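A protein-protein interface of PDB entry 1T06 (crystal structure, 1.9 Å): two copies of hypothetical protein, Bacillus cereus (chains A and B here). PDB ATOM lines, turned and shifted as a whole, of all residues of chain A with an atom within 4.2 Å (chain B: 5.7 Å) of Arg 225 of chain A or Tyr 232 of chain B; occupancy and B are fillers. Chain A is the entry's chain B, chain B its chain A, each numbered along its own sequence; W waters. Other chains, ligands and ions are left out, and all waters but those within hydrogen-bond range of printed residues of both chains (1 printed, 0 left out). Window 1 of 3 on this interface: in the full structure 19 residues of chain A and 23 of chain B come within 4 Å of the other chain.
Position printed for both chains: 230.
Arg 225 of chain A touches three residues of chain B. Of chain A, only Arg 223 and Arg 225 come within 4 Å of Tyr 232 of chain B. Of the printed residues of chain A, Tyr 22 of chain B touches Gly 224. Of the printed residues of chain B, Phe 228 of chain A touches Thr 36, Val 233 and Cys 235. Of the printed residues of chain A, Cys 235 of chain B touches Phe 228. Printed residues of chain A within 4 Å of Val 233 of chain B: Arg 225 (2.8 Å) and Phe 228 (3.3 Å). The nearest printed residue of chain A that does not touch Tyr 232 of chain B is Arg 230 of chain A (7.5 Å). The nearest printed residue of chain A that does not touch Ala 35 of chain B is Arg 225 of chain A (5.3 Å).
The backbone NH (N) of Thr 36 of chain B lies within hydrogen-bond range of the backbone carbonyl oxygen (O) of Gly 224 of chain A, at 3.3 Å. OH of Tyr 232 of chain B lies within hydrogen-bond range of NH1 of Arg 223 of chain A (3.1 Å). The guanidinium group (NH2) of Arg 225 of chain A is in hydrogen-bond range of the backbone carbonyl oxygen (O) of Val 233 of chain B, 2.8 Å away.
Water W1 lies within hydrogen-bond range of the backbone carbonyl oxygen (O) of Arg 223 of chain A (2.6 Å), the side-chain hydroxyl (OG1) of Thr 36 of chain B (2.7 Å), the backbone carbonyl oxygen (O) of Gly 224 of chain A (3.4 Å) and the guanidinium group (NE) of Arg 225 of chain A (3.4 Å).
Of the 9 printed residues of chain A, 5 touch a printed residue of chain B. Printed residues of chain A that touch a printed residue of chain B: Arg 223, Gly 224, Arg 225, Leu 226 and Phe 228. Along chain A the printed residues that touch a printed residue of chain B span positions 223 to 228. Hydrophobic or aromatic side chains of chain B within 4 Å of the printed part of chain A: Tyr 22, Ala 35, Tyr 97, Tyr 232 and Val 233. Among the printed residues, 12 pairs touch across the chains.
O of Glu 220 of chain A lies within hydrogen-bond range of N of Arg 225 of chain A (3.0 Å).
Among the printed residues, pairs that only touch across the chains: Phe 228 of chain A with Val 233 of chain B (3.3 Å), Arg 223 of chain A with Tyr 97 of chain B (3.3 Å), Leu 226 of chain A with Ala 35 of chain B (3.4 Å), Arg 225 of chain A with Thr 36 of chain B (3.5 Å), Gly 224 of chain A with Tyr 22 of chain B (3.5 Å), Gly 224 of chain A with Ala 35 of chain B (3.6 Å), Phe 228 of chain A with Cys 235 of chain B (3.6 Å), Arg 225 of chain A with Tyr 232 of chain B (3.8 Å) and Phe 228 of chain A with Thr 36 of chain B (3.9 Å).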
ATOM      1  N   ILE A 180      25.271 -11.594  37.839  1.00  0.00           N
ATOM      2  CA  ILE A 180      24.054 -11.652  37.033  1.00  0.00           C
ATOM      3  C   ILE A 180      23.157 -12.879  37.253  1.00  0.00           C
ATOM      4  O   ILE A 180      21.936 -12.748  37.308  1.00  0.00           O
ATOM      5  CB  ILE A 180      24.390 -11.559  35.516  1.00  0.00           C
ATOM      6  CG1 ILE A 180      25.055 -10.214  35.209  1.00  0.00           C
ATOM      7  CG2 ILE A 180      23.131 -11.717  34.680  1.00  0.00           C
ATOM      8  CD1 ILE A 180      24.209  -9.010  35.548  1.00  0.00           C
ATOM      9  N   GLU A 220      25.234  -6.018  31.221  1.00  0.00           N
ATOM     10  CA  GLU A 220      24.171  -7.007  31.382  1.00  0.00           C
ATOM     11  C   GLU A 220      22.982  -6.411  32.136  1.00  0.00           C
ATOM     12  O   GLU A 220      21.831  -6.613  31.746  1.00  0.00           O
ATOM     13  CB  GLU A 220      24.699  -8.239  32.113  1.00  0.00           C
ATOM     14  CG  GLU A 220      25.688  -9.014  31.281  1.00  0.00           C
ATOM     15  CD  GLU A 220      25.134  -9.338  29.901  1.00  0.00           C
ATOM     16  OE1 GLU A 220      24.223 -10.192  29.806  1.00  0.00           O
ATOM     17  OE2 GLU A 220      25.606  -8.725  28.913  1.00  0.00           O
ATOM     18  N   ARG A 223      20.732  -4.158  30.071  1.00  0.00           N
ATOM     19  CA  ARG A 223      19.807  -4.867  29.193  1.00  0.00           C
ATOM     20  C   ARG A 223      18.675  -5.555  29.970  1.00  0.00           C
ATOM     21  O   ARG A 223      17.765  -6.136  29.377  1.00  0.00           O
ATOM     22  CB  ARG A 223      20.586  -5.897  28.376  1.00  0.00           C
ATOM     23  CG  ARG A 223      19.777  -6.676  27.361  1.00  0.00           C
ATOM     24  CD  ARG A 223      20.642  -7.787  26.775  1.00  0.00           C
ATOM     25  NE  ARG A 223      21.885  -7.252  26.213  1.00  0.00           N
ATOM     26  CZ  ARG A 223      22.005  -6.775  24.976  1.00  0.00           C
ATOM     27  NH1 ARG A 223      20.960  -6.769  24.154  1.00  0.00           N
ATOM     28  NH2 ARG A 223      23.169  -6.288  24.564  1.00  0.00           N
ATOM     29  N   GLY A 224      18.734  -5.487  31.295  1.00  0.00           N
ATOM     30  CA  GLY A 224      17.705  -6.112  32.113  1.00  0.00           C
ATOM     31  C   GLY A 224      17.926  -7.602  32.279  1.00  0.00           C
ATOM     32  O   GLY A 224      16.964  -8.369  32.372  1.00  0.00           O
ATOM     33  N   ARG A 225      19.199  -8.004  32.325  1.00  0.00           N
ATOM     34  CA  ARG A 225      19.575  -9.410  32.473  1.00  0.00           C
ATOM     35  C   ARG A 225      19.820  -9.823  33.913  1.00  0.00           C
ATOM     36  O   ARG A 225      20.290 -10.925  34.163  1.00  0.00           O
ATOM     37  CB  ARG A 225      20.833  -9.729  31.664  1.00  0.00           C
ATOM     38  CG  ARG A 225      20.691  -9.610  30.153  1.00  0.00           C
ATOM     39  CD  ARG A 225      19.722 -10.626  29.569  1.00  0.00           C
ATOM     40  NE  ARG A 225      19.840 -10.662  28.108  1.00  0.00           N
ATOM     41  CZ  ARG A 225      18.984 -11.267  27.286  1.00  0.00           C
ATOM     42  NH1 ARG A 225      17.921 -11.901  27.771  1.00  0.00           N
ATOM     43  NH2 ARG A 225      19.190 -11.231  25.972  1.00  0.00           N
ATOM     44  N   LEU A 226      19.518  -8.954  34.864  1.00  0.00           N
ATOM     45  CA  LEU A 226      19.717  -9.335  36.251  1.00  0.00           C
ATOM     46  C   LEU A 226      18.910 -10.603  36.522  1.00  0.00           C
ATOM     47  O   LEU A 226      17.750 -10.707  36.120  1.00  0.00           O
ATOM     48  CB  LEU A 226      19.255  -8.233  37.198  1.00  0.00           C
ATOM     49  CG  LEU A 226      19.475  -8.618  38.665  1.00  0.00           C
ATOM     50  CD1 LEU A 226      20.970  -8.744  38.944  1.00  0.00           C
ATOM     51  CD2 LEU A 226      18.839  -7.580  39.577  1.00  0.00           C
ATOM     52  N   GLY A 227      19.529 -11.571  37.192  1.00  0.00           N
ATOM     53  CA  GLY A 227      18.844 -12.816  37.504  1.00  0.00           C
ATOM     54  C   GLY A 227      18.676 -13.735  36.309  1.00  0.00           C
ATOM     55  O   GLY A 227      18.080 -14.808  36.420  1.00  0.00           O
ATOM     56  N   PHE A 228      19.203 -13.327  35.161  1.00  0.00           N
ATOM     57  CA  PHE A 228      19.074 -14.149  33.973  1.00  0.00           C
ATOM     58  C   PHE A 228      19.985 -15.371  34.032  1.00  0.00           C
ATOM     59  O   PHE A 228      21.184 -15.260  34.286  1.00  0.00           O
ATOM     60  CB  PHE A 228      19.373 -13.335  32.713  1.00  0.00           C
ATOM     61  CG  PHE A 228      18.988 -14.042  31.452  1.00  0.00           C
ATOM     62  CD1 PHE A 228      19.855 -14.950  30.855  1.00  0.00           C
ATOM     63  CD2 PHE A 228      17.718 -13.863  30.902  1.00  0.00           C
ATOM     64  CE1 PHE A 228      19.464 -15.674  29.731  1.00  0.00           C
ATOM     65  CE2 PHE A 228      17.313 -14.582  29.777  1.00  0.00           C
ATOM     66  CZ  PHE A 228      18.189 -15.490  29.192  1.00  0.00           C
ATOM     67  N   ARG A 230      21.300 -18.488  31.802  1.00  0.00           N
ATOM     68  CA  ARG A 230      21.382 -19.086  30.479  1.00  0.00           C
ATOM     69  C   ARG A 230      22.196 -20.371  30.497  1.00  0.00           C
ATOM     70  O   ARG A 230      23.354 -20.386  30.906  1.00  0.00           O
ATOM     71  CB  ARG A 230      21.967 -18.096  29.465  1.00  0.00           C
ATOM     72  CG  ARG A 230      23.306 -17.503  29.835  1.00  0.00           C
ATOM     73  CD  ARG A 230      23.780 -16.557  28.735  1.00  0.00           C
ATOM     74  NE  ARG A 230      22.998 -15.322  28.665  1.00  0.00           N
ATOM     75  CZ  ARG A 230      22.513 -14.804  27.537  1.00  0.00           C
ATOM     76  NH1 ARG A 230      21.820 -13.672  27.567  1.00  0.00           N
ATOM     77  NH2 ARG A 230      22.705 -15.428  26.381  1.00  0.00           N
ATOM     78  N   TYR B  22      16.123   0.740  33.715  1.00  0.00           N
ATOM     79  CA  TYR B  22      15.367   1.005  32.491  1.00  0.00           C
ATOM     80  C   TYR B  22      15.109   2.494  32.312  1.00  0.00           C
ATOM     81  O   TYR B  22      15.256   3.035  31.211  1.00  0.00           O
ATOM     82  CB  TYR B  22      14.017   0.277  32.500  1.00  0.00           C
ATOM     83  CG  TYR B  22      14.093  -1.235  32.430  1.00  0.00           C
ATOM     84  CD1 TYR B  22      15.186  -1.875  31.851  1.00  0.00           C
ATOM     85  CD2 TYR B  22      13.050  -2.026  32.914  1.00  0.00           C
ATOM     86  CE1 TYR B  22      15.240  -3.275  31.759  1.00  0.00           C
ATOM     87  CE2 TYR B  22      13.091  -3.420  32.820  1.00  0.00           C
ATOM     88  CZ  TYR B  22      14.189  -4.039  32.244  1.00  0.00           C
ATOM     89  OH  TYR B  22      14.244  -5.415  32.163  1.00  0.00           O
ATOM     90  N   ALA B  35      12.740  -7.860  34.947  1.00  0.00           N
ATOM     91  CA  ALA B  35      13.906  -8.488  34.340  1.00  0.00           C
ATOM     92  C   ALA B  35      13.339  -9.516  33.356  1.00  0.00           C
ATOM     93  O   ALA B  35      12.427 -10.279  33.701  1.00  0.00           O
ATOM     94  CB  ALA B  35      14.758  -9.167  35.414  1.00  0.00           C
ATOM     95  N   THR B  36      13.879  -9.525  32.139  1.00  0.00           N
ATOM     96  CA  THR B  36      13.416 -10.404  31.066  1.00  0.00           C
ATOM     97  C   THR B  36      13.256 -11.887  31.388  1.00  0.00           C
ATOM     98  O   THR B  36      12.298 -12.519  30.941  1.00  0.00           O
ATOM     99  CB  THR B  36      14.322 -10.264  29.821  1.00  0.00           C
ATOM    100  OG1 THR B  36      15.667 -10.651  30.146  1.00  0.00           O
ATOM    101  CG2 THR B  36      14.321  -8.822  29.342  1.00  0.00           C
ATOM    102  N   TYR B  66       7.388  -4.800  25.957  1.00  0.00           N
ATOM    103  CA  TYR B  66       8.435  -5.790  25.721  1.00  0.00           C
ATOM    104  C   TYR B  66       7.791  -7.174  25.650  1.00  0.00           C
ATOM    105  O   TYR B  66       8.110  -7.984  24.774  1.00  0.00           O
ATOM    106  CB  TYR B  66       9.469  -5.769  26.851  1.00  0.00           C
ATOM    107  CG  TYR B  66      10.630  -6.712  26.602  1.00  0.00           C
ATOM    108  CD1 TYR B  66      11.801  -6.263  25.988  1.00  0.00           C
ATOM    109  CD2 TYR B  66      10.546  -8.064  26.959  1.00  0.00           C
ATOM    110  CE1 TYR B  66      12.864  -7.135  25.736  1.00  0.00           C
ATOM    111  CE2 TYR B  66      11.600  -8.946  26.711  1.00  0.00           C
ATOM    112  CZ  TYR B  66      12.757  -8.475  26.101  1.00  0.00           C
ATOM    113  OH  TYR B  66      13.805  -9.342  25.867  1.00  0.00           O
ATOM    114  N   TYR B  97      15.449  -4.074  20.820  1.00  0.00           N
ATOM    115  CA  TYR B  97      15.162  -5.367  21.434  1.00  0.00           C
ATOM    116  C   TYR B  97      13.726  -5.866  21.375  1.00  0.00           C
ATOM    117  O   TYR B  97      13.462  -7.023  21.721  1.00  0.00           O
ATOM    118  CB  TYR B  97      15.617  -5.365  22.901  1.00  0.00           C
ATOM    119  CG  TYR B  97      17.004  -4.797  23.131  1.00  0.00           C
ATOM    120  CD1 TYR B  97      18.031  -5.006  22.207  1.00  0.00           C
ATOM    121  CD2 TYR B  97      17.289  -4.052  24.278  1.00  0.00           C
ATOM    122  CE1 TYR B  97      19.312  -4.483  22.416  1.00  0.00           C
ATOM    123  CE2 TYR B  97      18.569  -3.523  24.502  1.00  0.00           C
ATOM    124  CZ  TYR B  97      19.574  -3.741  23.564  1.00  0.00           C
ATOM    125  OH  TYR B  97      20.834  -3.215  23.766  1.00  0.00           O
ATOM    126  N   VAL B 101      13.358  -7.263  16.948  1.00  0.00           N
ATOM    127  CA  VAL B 101      13.424  -8.709  17.115  1.00  0.00           C
ATOM    128  C   VAL B 101      12.153  -9.331  16.555  1.00  0.00           C
ATOM    129  O   VAL B 101      12.211 -10.376  15.911  1.00  0.00           O
ATOM    130  CB  VAL B 101      13.634  -9.140  18.599  1.00  0.00           C
ATOM    131  CG1 VAL B 101      14.938  -8.558  19.133  1.00  0.00           C
ATOM    132  CG2 VAL B 101      12.487  -8.679  19.446  1.00  0.00           C
ATOM    133  N   TRP B 134      19.720  -9.555  14.197  1.00  0.00           N
ATOM    134  CA  TRP B 134      18.911 -10.687  14.632  1.00  0.00           C
ATOM    135  C   TRP B 134      18.702 -11.658  13.476  1.00  0.00           C
ATOM    136  O   TRP B 134      18.729 -12.875  13.666  1.00  0.00           O
ATOM    137  CB  TRP B 134      17.565 -10.176  15.148  1.00  0.00           C
ATOM    138  CG  TRP B 134      17.693  -9.037  16.146  1.00  0.00           C
ATOM    139  CD1 TRP B 134      16.805  -8.013  16.333  1.00  0.00           C
ATOM    140  CD2 TRP B 134      18.768  -8.807  17.076  1.00  0.00           C
ATOM    141  NE1 TRP B 134      17.258  -7.165  17.314  1.00  0.00           N
ATOM    142  CE2 TRP B 134      18.459  -7.626  17.788  1.00  0.00           C
ATOM    143  CE3 TRP B 134      19.961  -9.485  17.378  1.00  0.00           C
ATOM    144  CZ2 TRP B 134      19.303  -7.102  18.787  1.00  0.00           C
ATOM    145  CZ3 TRP B 134      20.804  -8.962  18.374  1.00  0.00           C
ATOM    146  CH2 TRP B 134      20.467  -7.783  19.062  1.00  0.00           C
ATOM    147  N   ASN B 138      19.079 -15.714  13.000  1.00  0.00           N
ATOM    148  CA  ASN B 138      17.910 -16.556  12.715  1.00  0.00           C
ATOM    149  C   ASN B 138      17.996 -17.358  11.425  1.00  0.00           C
ATOM    150  O   ASN B 138      17.418 -18.436  11.338  1.00  0.00           O
ATOM    151  CB  ASN B 138      16.629 -15.710  12.618  1.00  0.00           C
ATOM    152  CG  ASN B 138      16.355 -14.902  13.868  1.00  0.00           C
ATOM    153  OD1 ASN B 138      17.148 -14.898  14.813  1.00  0.00           O
ATOM    154  ND2 ASN B 138      15.225 -14.198  13.875  1.00  0.00           N
ATOM    155  N   ARG B 230      22.322 -17.806  16.524  1.00  0.00           N
ATOM    156  CA  ARG B 230      21.266 -18.130  17.476  1.00  0.00           C
ATOM    157  C   ARG B 230      20.272 -16.981  17.523  1.00  0.00           C
ATOM    158  O   ARG B 230      20.649 -15.821  17.337  1.00  0.00           O
ATOM    159  CB  ARG B 230      21.847 -18.386  18.866  1.00  0.00           C
ATOM    160  CG  ARG B 230      22.290 -17.140  19.621  1.00  0.00           C
ATOM    161  CD  ARG B 230      23.346 -16.341  18.880  1.00  0.00           C
ATOM    162  NE  ARG B 230      23.962 -15.350  19.762  1.00  0.00           N
ATOM    163  CZ  ARG B 230      25.001 -14.585  19.430  1.00  0.00           C
ATOM    164  NH1 ARG B 230      25.550 -14.684  18.223  1.00  0.00           N
ATOM    165  NH2 ARG B 230      25.504 -13.733  20.317  1.00  0.00           N
ATOM    166  N   LYS B 231      19.001 -17.307  17.746  1.00  0.00           N
ATOM    167  CA  LYS B 231      17.962 -16.286  17.816  1.00  0.00           C
ATOM    168  C   LYS B 231      18.218 -15.434  19.049  1.00  0.00           C
ATOM    169  O   LYS B 231      18.871 -15.882  19.990  1.00  0.00           O
ATOM    170  CB  LYS B 231      16.582 -16.930  17.925  1.00  0.00           C
ATOM    171  CG  LYS B 231      16.306 -17.995  16.882  1.00  0.00           C
ATOM    172  CD  LYS B 231      14.923 -18.612  17.075  1.00  0.00           C
ATOM    173  CE  LYS B 231      13.809 -17.694  16.591  1.00  0.00           C
ATOM    174  NZ  LYS B 231      13.799 -17.524  15.106  1.00  0.00           N
ATOM    175  N   TYR B 232      17.720 -14.202  19.041  1.00  0.00           N
ATOM    176  CA  TYR B 232      17.897 -13.316  20.188  1.00  0.00           C
ATOM    177  C   TYR B 232      17.200 -13.969  21.381  1.00  0.00           C
ATOM    178  O   TYR B 232      16.102 -14.491  21.242  1.00  0.00           O
ATOM    179  CB  TYR B 232      17.278 -11.944  19.892  1.00  0.00           C
ATOM    180  CG  TYR B 232      17.477 -10.921  20.989  1.00  0.00           C
ATOM    181  CD1 TYR B 232      16.610 -10.849  22.077  1.00  0.00           C
ATOM    182  CD2 TYR B 232      18.555 -10.041  20.951  1.00  0.00           C
ATOM    183  CE1 TYR B 232      16.816  -9.919  23.106  1.00  0.00           C
ATOM    184  CE2 TYR B 232      18.773  -9.117  21.967  1.00  0.00           C
ATOM    185  CZ  TYR B 232      17.905  -9.058  23.043  1.00  0.00           C
ATOM    186  OH  TYR B 232      18.146  -8.150  24.052  1.00  0.00           O
ATOM    187  N   VAL B 233      17.848 -13.965  22.542  1.00  0.00           N
ATOM    188  CA  VAL B 233      17.255 -14.557  23.738  1.00  0.00           C
ATOM    189  C   VAL B 233      16.416 -13.485  24.411  1.00  0.00           C
ATOM    190  O   VAL B 233      16.950 -12.619  25.110  1.00  0.00           O
ATOM    191  CB  VAL B 233      18.330 -15.048  24.725  1.00  0.00           C
ATOM    192  CG1 VAL B 233      17.665 -15.584  25.982  1.00  0.00           C
ATOM    193  CG2 VAL B 233      19.175 -16.134  24.071  1.00  0.00           C
ATOM    194  N   ARG B 234      15.103 -13.561  24.195  1.00  0.00           N
ATOM    195  CA  ARG B 234      14.146 -12.589  24.718  1.00  0.00           C
ATOM    196  C   ARG B 234      13.782 -12.720  26.204  1.00  0.00           C
ATOM    197  O   ARG B 234      13.447 -11.727  26.855  1.00  0.00           O
ATOM    198  CB  ARG B 234      12.876 -12.637  23.855  1.00  0.00           C
ATOM    199  CG  ARG B 234      13.193 -12.668  22.357  1.00  0.00           C
ATOM    200  CD  ARG B 234      11.962 -12.637  21.478  1.00  0.00           C
ATOM    201  NE  ARG B 234      11.377 -11.303  21.400  1.00  0.00           N
ATOM    202  CZ  ARG B 234      10.478 -10.934  20.490  1.00  0.00           C
ATOM    203  NH1 ARG B 234      10.060 -11.799  19.576  1.00  0.00           N
ATOM    204  NH2 ARG B 234       9.999  -9.698  20.490  1.00  0.00           N
ATOM    205  N   CYS B 235      13.842 -13.936  26.737  1.00  0.00           N
ATOM    206  CA  CYS B 235      13.514 -14.170  28.142  1.00  0.00           C
ATOM    207  C   CYS B 235      14.003 -15.544  28.591  1.00  0.00           C
ATOM    208  O   CYS B 235      14.663 -16.226  27.782  1.00  0.00           O
ATOM    209  CB  CYS B 235      11.997 -14.067  28.356  1.00  0.00           C
ATOM    210  SG  CYS B 235      11.019 -15.323  27.481  1.00  0.00           S
ATOM    211  OXT CYS B 235      13.722 -15.927  29.747  1.00  0.00           O
HETATM  212  O   HOH W   1      17.219  -8.704  29.036  1.00  0.00           O
